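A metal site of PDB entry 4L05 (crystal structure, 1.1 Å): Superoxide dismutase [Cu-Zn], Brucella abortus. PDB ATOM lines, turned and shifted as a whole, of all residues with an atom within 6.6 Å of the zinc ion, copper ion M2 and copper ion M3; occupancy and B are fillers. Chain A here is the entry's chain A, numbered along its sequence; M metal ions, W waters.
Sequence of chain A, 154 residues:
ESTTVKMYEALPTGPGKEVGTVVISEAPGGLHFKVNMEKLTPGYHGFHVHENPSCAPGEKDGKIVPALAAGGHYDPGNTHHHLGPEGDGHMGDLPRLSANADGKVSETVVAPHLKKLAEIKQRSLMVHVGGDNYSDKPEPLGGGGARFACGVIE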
ATOM      1  N   GLY A  46      20.253 -22.999  18.935  1.00  0.00           N
ATOM      2  CA  GLY A  46      21.217 -22.042  19.451  1.00  0.00           C
ATOM      3  C   GLY A  46      22.475 -21.969  18.621  1.00  0.00           C
ATOM      4  O   GLY A  46      22.934 -22.976  18.050  1.00  0.00           O
ATOM      5  N   PHE A  47      23.042 -20.769  18.546  1.00  0.00           N
ATOM      6  CA  PHE A  47      24.162 -20.441  17.668  1.00  0.00           C
ATOM      7  C   PHE A  47      25.056 -19.454  18.384  1.00  0.00           C
ATOM      8  O   PHE A  47      24.624 -18.356  18.741  1.00  0.00           O
ATOM      9  CB  PHE A  47      23.569 -19.845  16.390  1.00  0.00           C
ATOM     10  CG  PHE A  47      24.576 -19.490  15.304  1.00  0.00           C
ATOM     11  CD1 PHE A  47      25.668 -20.283  15.021  1.00  0.00           C
ATOM     12  CD2 PHE A  47      24.341 -18.384  14.502  1.00  0.00           C
ATOM     13  CE1 PHE A  47      26.541 -19.958  13.991  1.00  0.00           C
ATOM     14  CE2 PHE A  47      25.203 -18.058  13.458  1.00  0.00           C
ATOM     15  CZ  PHE A  47      26.298 -18.867  13.203  1.00  0.00           C
ATOM     16  N   HIS A  48      26.304 -19.860  18.644  1.00  0.00           N
ATOM     17  CA  HIS A  48      27.206 -19.018  19.426  1.00  0.00           C
ATOM     18  C   HIS A  48      28.621 -19.138  18.915  1.00  0.00           C
ATOM     19  O   HIS A  48      29.037 -20.182  18.412  1.00  0.00           O
ATOM     20  CB  HIS A  48      27.227 -19.416  20.906  1.00  0.00           C
ATOM     21  CG  HIS A  48      25.919 -19.884  21.438  1.00  0.00           C
ATOM     22  ND1 HIS A  48      25.732 -21.192  21.852  1.00  0.00           N
ATOM     23  CD2 HIS A  48      24.748 -19.243  21.625  1.00  0.00           C
ATOM     24  CE1 HIS A  48      24.478 -21.322  22.253  1.00  0.00           C
ATOM     25  NE2 HIS A  48      23.863 -20.168  22.133  1.00  0.00           N
ATOM     26  N   VAL A  49      29.389 -18.072  19.114  1.00  0.00           N
ATOM     27  CA  VAL A  49      30.836 -18.127  19.007  1.00  0.00           C
ATOM     28  C   VAL A  49      31.383 -18.695  20.319  1.00  0.00           C
ATOM     29  O   VAL A  49      31.082 -18.171  21.398  1.00  0.00           O
ATOM     30  CB  VAL A  49      31.454 -16.745  18.769  1.00  0.00           C
ATOM     31  CG1 VAL A  49      32.971 -16.881  18.552  1.00  0.00           C
ATOM     32  CG2 VAL A  49      30.790 -16.033  17.595  1.00  0.00           C
ATOM     33  N   HIS A  50      32.146 -19.786  20.239  1.00  0.00           N
ATOM     34  CA  HIS A  50      32.815 -20.370  21.374  1.00  0.00           C
ATOM     35  C   HIS A  50      34.282 -19.933  21.393  1.00  0.00           C
ATOM     36  O   HIS A  50      34.797 -19.392  20.415  1.00  0.00           O
ATOM     37  CB  HIS A  50      32.647 -21.885  21.389  1.00  0.00           C
ATOM     38  CG  HIS A  50      31.281 -22.329  21.849  1.00  0.00           C
ATOM     39  ND1 HIS A  50      31.099 -23.169  22.911  1.00  0.00           N
ATOM     40  CD2 HIS A  50      30.041 -22.065  21.364  1.00  0.00           C
ATOM     41  CE1 HIS A  50      29.801 -23.398  23.079  1.00  0.00           C
ATOM     42  NE2 HIS A  50      29.134 -22.736  22.146  1.00  0.00           N
ATOM     43  N   GLY A  71      35.406 -25.084  24.113  1.00  0.00           N
ATOM     44  CA  GLY A  71      35.266 -24.272  25.305  1.00  0.00           C
ATOM     45  C   GLY A  71      33.868 -23.688  25.444  1.00  0.00           C
ATOM     46  O   GLY A  71      32.889 -24.146  24.817  1.00  0.00           O
ATOM     47  N   GLY A  72      33.773 -22.681  26.310  1.00  0.00           N
ATOM     48  CA  GLY A  72      32.527 -22.008  26.556  1.00  0.00           C
ATOM     49  C   GLY A  72      32.279 -20.916  25.534  1.00  0.00           C
ATOM     50  O   GLY A  72      32.965 -20.819  24.532  1.00  0.00           O
ATOM     51  N   HIS A  73      31.262 -20.100  25.775  1.00  0.00           N
ATOM     52  CA  HIS A  73      30.957 -18.999  24.873  1.00  0.00           C
ATOM     53  C   HIS A  73      32.033 -17.935  24.946  1.00  0.00           C
ATOM     54  O   HIS A  73      32.538 -17.613  26.026  1.00  0.00           O
ATOM     55  CB  HIS A  73      29.593 -18.400  25.229  1.00  0.00           C
ATOM     56  CG  HIS A  73      28.467 -19.376  25.079  1.00  0.00           C
ATOM     57  ND1 HIS A  73      27.136 -19.016  25.161  1.00  0.00           N
ATOM     58  CD2 HIS A  73      28.480 -20.698  24.824  1.00  0.00           C
ATOM     59  CE1 HIS A  73      26.390 -20.096  24.974  1.00  0.00           C
ATOM     60  NE2 HIS A  73      27.181 -21.126  24.780  1.00  0.00           N
ATOM     61  N   TYR A  74      32.378 -17.382  23.794  1.00  0.00           N
ATOM     62  CA  TYR A  74      33.308 -16.266  23.721  1.00  0.00           C
ATOM     63  C   TYR A  74      32.773 -15.149  24.623  1.00  0.00           C
ATOM     64  O   TYR A  74      31.628 -14.718  24.481  1.00  0.00           O
ATOM     65  CB  TYR A  74      33.461 -15.825  22.267  1.00  0.00           C
ATOM     66  CG  TYR A  74      34.244 -14.549  22.057  1.00  0.00           C
ATOM     67  CD1 TYR A  74      35.572 -14.442  22.445  1.00  0.00           C
ATOM     68  CD2 TYR A  74      33.640 -13.444  21.472  1.00  0.00           C
ATOM     69  CE1 TYR A  74      36.276 -13.266  22.241  1.00  0.00           C
ATOM     70  CE2 TYR A  74      34.334 -12.268  21.270  1.00  0.00           C
ATOM     71  CZ  TYR A  74      35.652 -12.189  21.657  1.00  0.00           C
ATOM     72  OH  TYR A  74      36.349 -11.014  21.483  1.00  0.00           O
ATOM     73  N   HIS A  81      27.798 -14.900  32.008  1.00  0.00           N
ATOM     74  CA  HIS A  81      26.389 -15.255  31.878  1.00  0.00           C
ATOM     75  C   HIS A  81      25.903 -14.987  30.459  1.00  0.00           C
ATOM     76  O   HIS A  81      26.499 -14.212  29.692  1.00  0.00           O
ATOM     77  CB  HIS A  81      25.516 -14.627  32.973  1.00  0.00           C
ATOM     78  CG  HIS A  81      25.517 -13.121  32.996  1.00  0.00           C
ATOM     79  ND1 HIS A  81      24.894 -12.411  33.988  1.00  0.00           N
ATOM     80  CD2 HIS A  81      26.034 -12.202  32.158  1.00  0.00           C
ATOM     81  CE1 HIS A  81      25.043 -11.123  33.776  1.00  0.00           C
ATOM     82  NE2 HIS A  81      25.727 -10.966  32.662  1.00  0.00           N
ATOM     83  N   HIS A  82      24.834 -15.695  30.104  1.00  0.00           N
ATOM     84  CA  HIS A  82      24.348 -15.797  28.744  1.00  0.00           C
ATOM     85  C   HIS A  82      23.116 -14.927  28.568  1.00  0.00           C
ATOM     86  O   HIS A  82      22.096 -15.197  29.174  1.00  0.00           O
ATOM     87  CB  HIS A  82      24.001 -17.277  28.509  1.00  0.00           C
ATOM     88  CG  HIS A  82      23.494 -17.577  27.131  1.00  0.00           C
ATOM     89  ND1 HIS A  82      24.323 -17.689  26.036  1.00  0.00           N
ATOM     90  CD2 HIS A  82      22.231 -17.745  26.686  1.00  0.00           C
ATOM     91  CE1 HIS A  82      23.577 -17.900  24.971  1.00  0.00           C
ATOM     92  NE2 HIS A  82      22.308 -17.937  25.327  1.00  0.00           N
ATOM     93  N   LEU A  83      23.208 -13.896  27.721  1.00  0.00           N
ATOM     94  CA  LEU A  83      22.117 -12.933  27.554  1.00  0.00           C
ATOM     95  C   LEU A  83      21.750 -12.664  26.107  1.00  0.00           C
ATOM     96  O   LEU A  83      20.931 -11.797  25.851  1.00  0.00           O
ATOM     97  CB  LEU A  83      22.412 -11.640  28.329  1.00  0.00           C
ATOM     98  CG  LEU A  83      22.415 -11.799  29.847  1.00  0.00           C
ATOM     99  CD1 LEU A  83      22.940 -10.523  30.519  1.00  0.00           C
ATOM    100  CD2 LEU A  83      21.046 -12.139  30.375  1.00  0.00           C
ATOM    101  N   GLY A  84      22.277 -13.440  25.159  1.00  0.00           N
ATOM    102  CA  GLY A  84      21.868 -13.300  23.784  1.00  0.00           C
ATOM    103  C   GLY A  84      22.527 -12.144  23.066  1.00  0.00           C
ATOM    104  O   GLY A  84      23.345 -11.386  23.620  1.00  0.00           O
ATOM    105  N   GLY A  89      25.857  -9.813  28.036  1.00  0.00           N
ATOM    106  CA  GLY A  89      26.569 -10.959  28.594  1.00  0.00           C
ATOM    107  C   GLY A  89      27.624 -11.420  27.614  1.00  0.00           C
ATOM    108  O   GLY A  89      28.309 -10.600  27.017  1.00  0.00           O
ATOM    109  N   HIS A  90      27.754 -12.743  27.418  1.00  0.00           N
ATOM    110  CA  HIS A  90      28.755 -13.256  26.491  1.00  0.00           C
ATOM    111  C   HIS A  90      28.666 -12.529  25.149  1.00  0.00           C
ATOM    112  O   HIS A  90      27.629 -12.569  24.477  1.00  0.00           O
ATOM    113  CB  HIS A  90      28.509 -14.718  26.160  1.00  0.00           C
ATOM    114  CG  HIS A  90      28.409 -15.653  27.331  1.00  0.00           C
ATOM    115  ND1 HIS A  90      27.511 -16.703  27.325  1.00  0.00           N
ATOM    116  CD2 HIS A  90      29.126 -15.770  28.475  1.00  0.00           C
ATOM    117  CE1 HIS A  90      27.666 -17.402  28.440  1.00  0.00           C
ATOM    118  NE2 HIS A  90      28.633 -16.853  29.149  1.00  0.00           N
ATOM    119  N   MET A  91      29.771 -11.931  24.707  1.00  0.00           N
ATOM    120  CA  MET A  91      29.768 -11.269  23.404  1.00  0.00           C
ATOM    121  C   MET A  91      29.650 -12.266  22.234  1.00  0.00           C
ATOM    122  O   MET A  91      29.296 -11.866  21.117  1.00  0.00           O
ATOM    123  CB  MET A  91      30.989 -10.374  23.222  1.00  0.00           C
ATOM    124  CG  MET A  91      30.703  -9.166  22.328  1.00  0.00           C
ATOM    125  SD  MET A  91      31.983  -7.917  22.343  1.00  0.00           S
ATOM    126  CE  MET A  91      32.046  -7.503  24.084  1.00  0.00           C
ATOM    127  N   GLY A  92      29.927 -13.532  22.480  1.00  0.00           N
ATOM    128  CA  GLY A  92      29.775 -14.556  21.462  1.00  0.00           C
ATOM    129  C   GLY A  92      28.343 -15.000  21.211  1.00  0.00           C
ATOM    130  O   GLY A  92      28.117 -15.852  20.356  1.00  0.00           O
ATOM    131  N   ASP A  93      27.381 -14.467  21.935  1.00  0.00           N
ATOM    132  CA  ASP A  93      25.990 -14.899  21.779  1.00  0.00           C
ATOM    133  C   ASP A  93      25.394 -14.353  20.479  1.00  0.00           C
ATOM    134  O   ASP A  93      25.295 -13.137  20.292  1.00  0.00           O
ATOM    135  CB  ASP A  93      25.159 -14.430  22.978  1.00  0.00           C
ATOM    136  CG  ASP A  93      25.484 -15.161  24.273  1.00  0.00           C
ATOM    137  OD1 ASP A  93      26.279 -16.147  24.215  1.00  0.00           O
ATOM    138  OD2 ASP A  93      24.929 -14.778  25.319  1.00  0.00           O
ATOM    139  N   MET A 126      29.431 -22.602  16.853  1.00  0.00           N
ATOM    140  CA  MET A 126      28.709 -23.752  17.351  1.00  0.00           C
ATOM    141  C   MET A 126      27.218 -23.622  17.059  1.00  0.00           C
ATOM    142  O   MET A 126      26.607 -22.571  17.342  1.00  0.00           O
ATOM    143  CB  MET A 126      28.881 -23.861  18.859  1.00  0.00           C
ATOM    144  CG  MET A 126      28.569 -25.223  19.421  1.00  0.00           C
ATOM    145  SD  MET A 126      29.852 -26.437  19.019  1.00  0.00           S
ATOM    146  CE  MET A 126      31.239 -25.751  19.901  1.00  0.00           C
ATOM    147  N   VAL A 127      26.626 -24.690  16.529  1.00  0.00           N
ATOM    148  CA  VAL A 127      25.179 -24.821  16.438  1.00  0.00           C
ATOM    149  C   VAL A 127      24.776 -25.941  17.387  1.00  0.00           C
ATOM    150  O   VAL A 127      25.389 -27.014  17.403  1.00  0.00           O
ATOM    151  CB  VAL A 127      24.734 -25.082  14.991  1.00  0.00           C
ATOM    152  CG1 VAL A 127      23.221 -25.299  14.933  1.00  0.00           C
ATOM    153  CG2 VAL A 127      25.134 -23.922  14.101  1.00  0.00           C
ATOM    154  N   HIS A 128      23.755 -25.687  18.201  1.00  0.00           N
ATOM    155  CA  HIS A 128      23.329 -26.618  19.236  1.00  0.00           C
ATOM    156  C   HIS A 128      22.125 -27.446  18.828  1.00  0.00           C
ATOM    157  O   HIS A 128      21.399 -27.109  17.892  1.00  0.00           O
ATOM    158  CB  HIS A 128      23.016 -25.823  20.503  1.00  0.00           C
ATOM    159  CG  HIS A 128      24.243 -25.323  21.191  1.00  0.00           C
ATOM    160  ND1 HIS A 128      24.850 -26.003  22.215  1.00  0.00           N
ATOM    161  CD2 HIS A 128      24.996 -24.224  20.972  1.00  0.00           C
ATOM    162  CE1 HIS A 128      25.924 -25.338  22.611  1.00  0.00           C
ATOM    163  NE2 HIS A 128      26.038 -24.254  21.877  1.00  0.00           N
ATOM    164  N   ASP A 132      17.620 -21.412  21.975  1.00  0.00           N
ATOM    165  CA  ASP A 132      18.289 -20.393  22.752  1.00  0.00           C
ATOM    166  C   ASP A 132      17.273 -19.357  23.198  1.00  0.00           C
ATOM    167  O   ASP A 132      16.778 -18.577  22.386  1.00  0.00           O
ATOM    168  CB  ASP A 132      19.382 -19.712  21.916  1.00  0.00           C
ATOM    169  CG  ASP A 132      20.361 -18.913  22.760  1.00  0.00           C
ATOM    170  OD1 ASP A 132      20.042 -18.604  23.935  1.00  0.00           O
ATOM    171  OD2 ASP A 132      21.452 -18.576  22.262  1.00  0.00           O
ATOM    172  N   LEU A 141      22.779 -21.460  29.582  1.00  0.00           N
ATOM    173  CA  LEU A 141      23.286 -21.247  28.224  1.00  0.00           C
ATOM    174  C   LEU A 141      22.160 -21.305  27.191  1.00  0.00           C
ATOM    175  O   LEU A 141      22.306 -21.837  26.078  1.00  0.00           O
ATOM    176  CB  LEU A 141      24.396 -22.259  27.911  1.00  0.00           C
ATOM    177  CG  LEU A 141      25.603 -22.149  28.860  1.00  0.00           C
ATOM    178  CD1 LEU A 141      26.465 -23.358  28.745  1.00  0.00           C
ATOM    179  CD2 LEU A 141      26.424 -20.925  28.531  1.00  0.00           C
ATOM    180  N   GLY A 142      21.031 -20.748  27.578  1.00  0.00           N
ATOM    181  CA  GLY A 142      19.898 -20.606  26.686  1.00  0.00           C
ATOM    182  C   GLY A 142      19.115 -21.874  26.419  1.00  0.00           C
ATOM    183  O   GLY A 142      18.193 -21.867  25.607  1.00  0.00           O
ATOM    184  N   GLY A 144      20.557 -24.473  25.062  1.00  0.00           N
ATOM    185  CA  GLY A 144      21.126 -25.035  23.853  1.00  0.00           C
ATOM    186  C   GLY A 144      21.494 -26.502  23.990  1.00  0.00           C
ATOM    187  O   GLY A 144      21.494 -27.250  23.000  1.00  0.00           O
ATOM    188  N   GLY A 145      21.827 -26.948  25.193  1.00  0.00           N
ATOM    189  CA  GLY A 145      22.180 -28.332  25.391  1.00  0.00           C
ATOM    190  C   GLY A 145      23.358 -28.753  24.526  1.00  0.00           C
ATOM    191  O   GLY A 145      24.342 -28.016  24.379  1.00  0.00           O
ATOM    192  N   ARG A 147      26.016 -30.006  21.649  1.00  0.00           N
ATOM    193  CA  ARG A 147      26.600 -29.360  20.482  1.00  0.00           C
ATOM    194  C   ARG A 147      26.345 -30.229  19.260  1.00  0.00           C
ATOM    195  O   ARG A 147      26.731 -31.379  19.219  1.00  0.00           O
ATOM    196  CB  ARG A 147      28.096 -29.171  20.747  1.00  0.00           C
ATOM    197  CG  ARG A 147      28.306 -28.230  21.934  1.00  0.00           C
ATOM    198  CD  ARG A 147      29.723 -28.163  22.489  1.00  0.00           C
ATOM    199  NE  ARG A 147      29.708 -27.380  23.723  1.00  0.00           N
ATOM    200  CZ  ARG A 147      30.723 -26.670  24.233  1.00  0.00           C
ATOM    201  NH1 ARG A 147      31.908 -26.619  23.653  1.00  0.00           N
ATOM    202  NH2 ARG A 147      30.516 -25.976  25.351  1.00  0.00           N
HETATM  203 ZN    ZN M   1      26.325 -17.312  25.783  1.00  0.00          ZN
HETATM  204 CU    CU M   2      27.060 -22.524  22.801  1.00  0.00          CU
HETATM  205 CU    CU M   3      27.192 -22.543  22.061  1.00  0.00          CU
HETATM  206  O   HOH W   1      27.013 -23.603  24.545  1.00  0.00           O
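NE2 of His 50 is bound to copper ion M3 (2.0 Å).
ND1 of His 48 binds copper ion M3, 2.0 Å away.
NE2 of His 128 binds copper ion M3, 2.1 Å away.
Slightly farther from copper ion M3 lies water W1 (2.7 Å).
The zinc ion is bound by the side-chain carboxylate (OD1) of Asp 93 (2.0 Å), a ring nitrogen (ND1) of His 73 (2.0 Å), a ring nitrogen (ND1) of His 90 (2.0 Å) and a ring nitrogen (ND1) of His 82 (2.1 Å).
The zinc ion has four donor atoms within binding distance.
Four residues have an atom within 4 Å of copper ion M2: His 48, His 50, His 73 and His 128.
Residues that only touch copper ion M3: Met 126.
Five residues have an atom within 4 Å of copper ion M3: His 48, His 50, His 73, Met 126 and His 128.
The nearest printed residue that does not touch copper ion M3 is Phe 47 (5.3 Å).
Water W1 is bound to copper ion M2, 2.1 Å away.
ND1 of His 48 is bound to copper ion M2 (2.1 Å).
A ring nitrogen (NE2) of His 50 binds copper ion M2, at 2.2 Å.
NE2 of His 128 is bound to copper ion M2, at 2.2 Å.
NE2 of His 73 binds copper ion M2.
The nearest printed residue that does not touch the zinc ion is Leu 141 (4.5 Å).
OD2 of Asp 93 is in hydrogen-bond range of N of Gly 84 (3.0 Å).
The backbone NH of His 90 sits at hydrogen-bond distance from the backbone carbonyl oxygen of His 81 (3.0 Å).
NE2 of His 48 lies within hydrogen-bond range of OD2 of Asp 132 (2.9 Å).
A ring nitrogen (ND1) of His 50 lies within hydrogen-bond range of the backbone carbonyl oxygen (O) of Gly 71, at 2.8 Å.
The side-chain carboxylate (OD1) of Asp 132 is in hydrogen-bond range of a ring nitrogen (NE2) of His 82 (2.7 Å).
The backbone carbonyl oxygen of Gly 46 sits at hydrogen-bond distance from the backbone NH of His 128 (2.8 Å).
The side-chain carboxylate of Asp 93 lies within hydrogen-bond range of the backbone NH of Leu 83 (3.1 Å).
ND1 of His 128 is in hydrogen-bond range of O of Gly 145 (3.0 Å).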
